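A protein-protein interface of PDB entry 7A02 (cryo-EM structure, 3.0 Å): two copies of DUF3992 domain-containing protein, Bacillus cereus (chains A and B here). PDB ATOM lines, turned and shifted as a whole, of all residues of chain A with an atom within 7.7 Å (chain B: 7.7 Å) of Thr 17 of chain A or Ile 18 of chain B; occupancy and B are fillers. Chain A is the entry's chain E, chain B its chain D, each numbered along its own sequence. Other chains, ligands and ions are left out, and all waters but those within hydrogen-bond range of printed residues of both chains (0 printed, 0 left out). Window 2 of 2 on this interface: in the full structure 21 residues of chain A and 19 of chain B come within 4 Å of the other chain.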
ATOM      1  N   GLY A  14      29.954  12.937  30.483  1.00  0.00           N
ATOM      2  CA  GLY A  14      30.541  14.213  30.137  1.00  0.00           C
ATOM      3  C   GLY A  14      29.721  15.004  29.146  1.00  0.00           C
ATOM      4  O   GLY A  14      28.600  15.421  29.453  1.00  0.00           O
ATOM      5  N   GLN A  15      30.276  15.228  27.958  1.00  0.00           N
ATOM      6  CA  GLN A  15      29.580  16.003  26.943  1.00  0.00           C
ATOM      7  C   GLN A  15      28.294  15.301  26.528  1.00  0.00           C
ATOM      8  O   GLN A  15      28.243  14.073  26.408  1.00  0.00           O
ATOM      9  CB  GLN A  15      30.484  16.231  25.731  1.00  0.00           C
ATOM     10  CG  GLN A  15      30.646  15.028  24.815  1.00  0.00           C
ATOM     11  CD  GLN A  15      31.665  14.030  25.327  1.00  0.00           C
ATOM     12  OE1 GLN A  15      32.040  14.051  26.499  1.00  0.00           O
ATOM     13  NE2 GLN A  15      32.117  13.144  24.447  1.00  0.00           N
ATOM     14  N   LYS A  16      27.245  16.089  26.335  1.00  0.00           N
ATOM     15  CA  LYS A  16      25.941  15.582  25.946  1.00  0.00           C
ATOM     16  C   LYS A  16      25.525  16.232  24.639  1.00  0.00           C
ATOM     17  O   LYS A  16      25.628  17.451  24.483  1.00  0.00           O
ATOM     18  CB  LYS A  16      24.897  15.860  27.024  1.00  0.00           C
ATOM     19  CG  LYS A  16      25.325  15.432  28.410  1.00  0.00           C
ATOM     20  CD  LYS A  16      24.412  16.011  29.471  1.00  0.00           C
ATOM     21  CE  LYS A  16      24.990  15.803  30.858  1.00  0.00           C
ATOM     22  NZ  LYS A  16      26.452  16.083  30.890  1.00  0.00           N
ATOM     23  N   THR A  17      25.060  15.416  23.707  1.00  0.00           N
ATOM     24  CA  THR A  17      24.610  15.894  22.413  1.00  0.00           C
ATOM     25  C   THR A  17      23.092  15.931  22.362  1.00  0.00           C
ATOM     26  O   THR A  17      22.404  15.224  23.100  1.00  0.00           O
ATOM     27  CB  THR A  17      25.140  15.004  21.297  1.00  0.00           C
ATOM     28  OG1 THR A  17      24.618  13.688  21.475  1.00  0.00           O
ATOM     29  CG2 THR A  17      26.649  14.946  21.344  1.00  0.00           C
ATOM     30  N   ILE A  18      22.577  16.766  21.471  1.00  0.00           N
ATOM     31  CA  ILE A  18      21.146  16.931  21.279  1.00  0.00           C
ATOM     32  C   ILE A  18      20.755  16.228  19.994  1.00  0.00           C
ATOM     33  O   ILE A  18      21.411  16.401  18.961  1.00  0.00           O
ATOM     34  CB  ILE A  18      20.765  18.416  21.229  1.00  0.00           C
ATOM     35  CG1 ILE A  18      21.091  19.072  22.556  1.00  0.00           C
ATOM     36  CG2 ILE A  18      19.300  18.576  20.933  1.00  0.00           C
ATOM     37  CD1 ILE A  18      20.991  20.548  22.506  1.00  0.00           C
ATOM     38  N   VAL A  19      19.693  15.426  20.052  1.00  0.00           N
ATOM     39  CA  VAL A  19      19.257  14.662  18.896  1.00  0.00           C
ATOM     40  C   VAL A  19      17.782  14.927  18.647  1.00  0.00           C
ATOM     41  O   VAL A  19      17.039  15.347  19.538  1.00  0.00           O
ATOM     42  CB  VAL A  19      19.516  13.158  19.071  1.00  0.00           C
ATOM     43  CG1 VAL A  19      20.991  12.903  19.239  1.00  0.00           C
ATOM     44  CG2 VAL A  19      18.774  12.650  20.260  1.00  0.00           C
ATOM     45  N   GLN A  20      17.366  14.673  17.406  1.00  0.00           N
ATOM     46  CA  GLN A  20      16.026  14.981  16.936  1.00  0.00           C
ATOM     47  C   GLN A  20      15.436  13.793  16.192  1.00  0.00           C
ATOM     48  O   GLN A  20      16.121  13.119  15.422  1.00  0.00           O
ATOM     49  CB  GLN A  20      16.036  16.190  16.022  1.00  0.00           C
ATOM     50  CG  GLN A  20      14.691  16.818  15.834  1.00  0.00           C
ATOM     51  CD  GLN A  20      14.771  18.075  15.025  1.00  0.00           C
ATOM     52  OE1 GLN A  20      15.661  18.231  14.199  1.00  0.00           O
ATOM     53  NE2 GLN A  20      13.847  18.989  15.258  1.00  0.00           N
ATOM     54  N   TYR A 114      15.677  15.660  22.154  1.00  0.00           N
ATOM     55  CA  TYR A 114      16.109  15.285  23.491  1.00  0.00           C
ATOM     56  C   TYR A 114      17.626  15.278  23.542  1.00  0.00           C
ATOM     57  O   TYR A 114      18.291  14.864  22.590  1.00  0.00           O
ATOM     58  CB  TYR A 114      15.536  13.936  23.940  1.00  0.00           C
ATOM     59  CG  TYR A 114      15.649  12.812  22.950  1.00  0.00           C
ATOM     60  CD1 TYR A 114      14.800  12.730  21.866  1.00  0.00           C
ATOM     61  CD2 TYR A 114      16.586  11.815  23.117  1.00  0.00           C
ATOM     62  CE1 TYR A 114      14.898  11.706  20.970  1.00  0.00           C
ATOM     63  CE2 TYR A 114      16.688  10.785  22.227  1.00  0.00           C
ATOM     64  CZ  TYR A 114      15.842  10.736  21.153  1.00  0.00           C
ATOM     65  OH  TYR A 114      15.938   9.706  20.254  1.00  0.00           O
ATOM     66  N   THR A 115      18.158  15.786  24.643  1.00  0.00           N
ATOM     67  CA  THR A 115      19.592  15.988  24.832  1.00  0.00           C
ATOM     68  C   THR A 115      20.241  14.842  25.587  1.00  0.00           C
ATOM     69  O   THR A 115      20.971  15.056  26.549  1.00  0.00           O
ATOM     70  CB  THR A 115      19.831  17.311  25.550  1.00  0.00           C
ATOM     71  OG1 THR A 115      21.227  17.458  25.837  1.00  0.00           O
ATOM     72  CG2 THR A 115      19.019  17.386  26.839  1.00  0.00           C
ATOM     73  N   LEU A 116      20.016  13.607  25.162  1.00  0.00           N
ATOM     74  CA  LEU A 116      20.625  12.476  25.847  1.00  0.00           C
ATOM     75  C   LEU A 116      21.592  11.719  24.952  1.00  0.00           C
ATOM     76  O   LEU A 116      22.780  11.628  25.273  1.00  0.00           O
ATOM     77  CB  LEU A 116      19.531  11.546  26.377  1.00  0.00           C
ATOM     78  CG  LEU A 116      18.792  12.047  27.618  1.00  0.00           C
ATOM     79  CD1 LEU A 116      17.347  11.580  27.615  1.00  0.00           C
ATOM     80  CD2 LEU A 116      19.502  11.583  28.880  1.00  0.00           C
ATOM     81  N   SER A 117      21.127  11.203  23.825  1.00  0.00           N
ATOM     82  CA  SER A 117      21.963  10.411  22.948  1.00  0.00           C
ATOM     83  C   SER A 117      21.272  10.210  21.616  1.00  0.00           C
ATOM     84  O   SER A 117      20.548   9.234  21.439  1.00  0.00           O
ATOM     85  CB  SER A 117      22.272   9.056  23.568  1.00  0.00           C
ATOM     86  OG  SER A 117      21.168   8.187  23.419  1.00  0.00           O
ATOM     87  N   LYS B  16      32.826   8.924  21.526  1.00  0.00           N
ATOM     88  CA  LYS B  16      31.740   8.019  21.198  1.00  0.00           C
ATOM     89  C   LYS B  16      30.771   8.721  20.265  1.00  0.00           C
ATOM     90  O   LYS B  16      30.379   9.864  20.511  1.00  0.00           O
ATOM     91  CB  LYS B  16      31.013   7.552  22.454  1.00  0.00           C
ATOM     92  CG  LYS B  16      31.935   7.030  23.534  1.00  0.00           C
ATOM     93  CD  LYS B  16      31.209   6.887  24.857  1.00  0.00           C
ATOM     94  CE  LYS B  16      32.187   6.618  25.986  1.00  0.00           C
ATOM     95  NZ  LYS B  16      33.395   7.481  25.880  1.00  0.00           N
ATOM     96  N   THR B  17      30.391   8.036  19.199  1.00  0.00           N
ATOM     97  CA  THR B  17      29.457   8.571  18.226  1.00  0.00           C
ATOM     98  C   THR B  17      28.080   7.964  18.428  1.00  0.00           C
ATOM     99  O   THR B  17      27.927   6.876  18.984  1.00  0.00           O
ATOM    100  CB  THR B  17      29.938   8.293  16.808  1.00  0.00           C
ATOM    101  OG1 THR B  17      29.999   6.880  16.615  1.00  0.00           O
ATOM    102  CG2 THR B  17      31.315   8.878  16.597  1.00  0.00           C
ATOM    103  N   ILE B  18      27.071   8.685  17.959  1.00  0.00           N
ATOM    104  CA  ILE B  18      25.684   8.262  18.059  1.00  0.00           C
ATOM    105  C   ILE B  18      25.232   7.791  16.690  1.00  0.00           C
ATOM    106  O   ILE B  18      25.464   8.474  15.687  1.00  0.00           O
ATOM    107  CB  ILE B  18      24.795   9.403  18.568  1.00  0.00           C
ATOM    108  CG1 ILE B  18      25.219   9.794  19.970  1.00  0.00           C
ATOM    109  CG2 ILE B  18      23.350   8.986  18.576  1.00  0.00           C
ATOM    110  CD1 ILE B  18      24.583  11.049  20.433  1.00  0.00           C
ATOM    111  N   VAL B  19      24.592   6.625  16.642  1.00  0.00           N
ATOM    112  CA  VAL B  19      24.157   6.052  15.380  1.00  0.00           C
ATOM    113  C   VAL B  19      22.678   5.710  15.467  1.00  0.00           C
ATOM    114  O   VAL B  19      22.115   5.542  16.552  1.00  0.00           O
ATOM    115  CB  VAL B  19      24.979   4.811  15.000  1.00  0.00           C
ATOM    116  CG1 VAL B  19      26.430   5.181  14.841  1.00  0.00           C
ATOM    117  CG2 VAL B  19      24.834   3.763  16.052  1.00  0.00           C
ATOM    118  N   GLN B  20      22.054   5.611  14.295  1.00  0.00           N
ATOM    119  CA  GLN B  20      20.620   5.416  14.170  1.00  0.00           C
ATOM    120  C   GLN B  20      20.315   4.310  13.173  1.00  0.00           C
ATOM    121  O   GLN B  20      20.954   4.201  12.126  1.00  0.00           O
ATOM    122  CB  GLN B  20      19.936   6.694  13.723  1.00  0.00           C
ATOM    123  CG  GLN B  20      18.462   6.710  13.968  1.00  0.00           C
ATOM    124  CD  GLN B  20      17.853   8.034  13.623  1.00  0.00           C
ATOM    125  OE1 GLN B  20      18.357   8.751  12.768  1.00  0.00           O
ATOM    126  NE2 GLN B  20      16.765   8.376  14.290  1.00  0.00           N
ATOM    127  N   ILE B 112      15.834   3.712  15.951  1.00  0.00           N
ATOM    128  CA  ILE B 112      16.562   3.359  17.161  1.00  0.00           C
ATOM    129  C   ILE B 112      17.870   4.131  17.195  1.00  0.00           C
ATOM    130  O   ILE B 112      18.613   4.134  16.213  1.00  0.00           O
ATOM    131  CB  ILE B 112      16.837   1.848  17.215  1.00  0.00           C
ATOM    132  CG1 ILE B 112      15.529   1.075  17.111  1.00  0.00           C
ATOM    133  CG2 ILE B 112      17.568   1.488  18.473  1.00  0.00           C
ATOM    134  CD1 ILE B 112      15.684  -0.282  16.499  1.00  0.00           C
ATOM    135  N   ARG B 113      18.158   4.771  18.321  1.00  0.00           N
ATOM    136  CA  ARG B 113      19.407   5.490  18.516  1.00  0.00           C
ATOM    137  C   ARG B 113      20.238   4.798  19.581  1.00  0.00           C
ATOM    138  O   ARG B 113      19.727   4.450  20.647  1.00  0.00           O
ATOM    139  CB  ARG B 113      19.157   6.929  18.945  1.00  0.00           C
ATOM    140  CG  ARG B 113      19.158   7.918  17.827  1.00  0.00           C
ATOM    141  CD  ARG B 113      18.692   9.260  18.329  1.00  0.00           C
ATOM    142  NE  ARG B 113      18.381  10.198  17.257  1.00  0.00           N
ATOM    143  CZ  ARG B 113      19.253  10.647  16.365  1.00  0.00           C
ATOM    144  NH1 ARG B 113      20.520  10.268  16.405  1.00  0.00           N
ATOM    145  NH2 ARG B 113      18.855  11.498  15.436  1.00  0.00           N
ATOM    146  N   TYR B 114      21.520   4.601  19.301  1.00  0.00           N
ATOM    147  CA  TYR B 114      22.413   4.137  20.351  1.00  0.00           C
ATOM    148  C   TYR B 114      23.780   4.768  20.158  1.00  0.00           C
ATOM    149  O   TYR B 114      24.256   4.923  19.032  1.00  0.00           O
ATOM    150  CB  TYR B 114      22.516   2.607  20.407  1.00  0.00           C
ATOM    151  CG  TYR B 114      22.745   1.917  19.093  1.00  0.00           C
ATOM    152  CD1 TYR B 114      21.717   1.742  18.191  1.00  0.00           C
ATOM    153  CD2 TYR B 114      23.986   1.410  18.770  1.00  0.00           C
ATOM    154  CE1 TYR B 114      21.923   1.110  17.001  1.00  0.00           C
ATOM    155  CE2 TYR B 114      24.198   0.771  17.581  1.00  0.00           C
ATOM    156  CZ  TYR B 114      23.165   0.626  16.700  1.00  0.00           C
ATOM    157  OH  TYR B 114      23.370  -0.014  15.505  1.00  0.00           O
ATOM    158  N   THR B 115      24.378   5.173  21.270  1.00  0.00           N
ATOM    159  CA  THR B 115      25.634   5.919  21.289  1.00  0.00           C
ATOM    160  C   THR B 115      26.835   5.016  21.506  1.00  0.00           C
ATOM    161  O   THR B 115      27.676   5.285  22.358  1.00  0.00           O
ATOM    162  CB  THR B 115      25.569   6.999  22.361  1.00  0.00           C
ATOM    163  OG1 THR B 115      26.839   7.657  22.460  1.00  0.00           O
ATOM    164  CG2 THR B 115      25.179   6.406  23.711  1.00  0.00           C
ATOM    165  N   LEU B 116      26.962   3.947  20.734  1.00  0.00           N
ATOM    166  CA  LEU B 116      28.103   3.059  20.897  1.00  0.00           C
ATOM    167  C   LEU B 116      28.988   3.030  19.661  1.00  0.00           C
ATOM    168  O   LEU B 116      30.167   3.382  19.744  1.00  0.00           O
ATOM    169  CB  LEU B 116      27.612   1.651  21.250  1.00  0.00           C
ATOM    170  CG  LEU B 116      27.121   1.471  22.686  1.00  0.00           C
ATOM    171  CD1 LEU B 116      26.003   0.447  22.753  1.00  0.00           C
ATOM    172  CD2 LEU B 116      28.274   1.067  23.592  1.00  0.00           C
ATOM    173  N   SER B 117      28.444   2.653  18.514  1.00  0.00           N
ATOM    174  CA  SER B 117      29.230   2.532  17.303  1.00  0.00           C
ATOM    175  C   SER B 117      28.316   2.382  16.106  1.00  0.00           C
ATOM    176  O   SER B 117      27.974   1.266  15.729  1.00  0.00           O
ATOM    177  CB  SER B 117      30.167   1.336  17.380  1.00  0.00           C
ATOM    178  OG  SER B 117      29.456   0.142  17.121  1.00  0.00           O
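OG1 of Thr 17 of chain A touches CD1 of Ile 18 of chain B, 2.8 Å away.
Arg 113 of chain B touches Val 19 of chain A (NE to CB, 3.7 Å).
Tyr 114 of chain A touches Arg 113 of chain B (OH to CD, 3.4 Å).
Ile 18 of chain B touches Ser 117 of chain A (CD1 to C, 3.6 Å).
Ser 117 of chain A touches Arg 113 of chain B.
Ser 117 of chain A touches Thr 115 of chain B (CB to CG2, 3.9 Å).
Thr 17 of chain A touches Ile 18 of chain B, but with the chains exchanged Ile 18 of chain A does not touch Thr 17 of chain B (10.8 Å).
Ser 117 of chain A touches Ile 18 of chain B, but with the chains exchanged Ile 18 of chain A does not touch Ser 117 of chain B (15.4 Å).
Ser 117 of chain A touches Thr 115 of chain B, but with the chains exchanged Thr 115 of chain A does not touch Ser 117 of chain B (16.3 Å).
Positions printed for both chains: 16, 17, 18, 19, 20, 114, 115, 116 and 117.
Of the 7 pairs that touch across the chains among the printed residues, none has its exchanged pair printed and touching as well.
O of Tyr 114 of chain A lies within hydrogen-bond range of N of Val 19 of chain A, 3.0 Å away.
Of the 11 printed residues of chain B, 3 touch a printed residue of chain A.
Hydrophobic or aromatic side chains of chain B within 4 Å of the printed part of chain A: Ile 18.
Along chain B the printed residues that touch a printed residue of chain A span positions 18 to 115.
Of the 11 printed residues of chain A, 5 touch a printed residue of chain B.
Hydrophobic or aromatic side chains of chain A that line the printed part of chain B: Val 19 and Tyr 114.
Among the printed residues, 7 pairs touch across the chains.
Of chain B, only Ile 18 comes within 4 Å of Thr 17 of chain A.
Ile 18 of chain B touches two residues of chain A.
Printed residues of chain B within 4 Å of Tyr 114 of chain A: Arg 113.
Printed residues of chain B within 4 Å of Gln 20 of chain A: Arg 113 (3.2 Å).
Printed residues of chain A within 4 Å of Thr 115 of chain B: Ser 117 (3.9 Å).
Of the printed residues of chain B, Val 19 of chain A touches Arg 113 (3.7 Å).
Tyr 114 of chain B touches none of the printed residues of chain A.
The backbone carbonyl oxygen (O) of Gln 20 of chain A is in hydrogen-bond range of the guanidinium group (NH2) of Arg 113 of chain B (3.2 Å).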
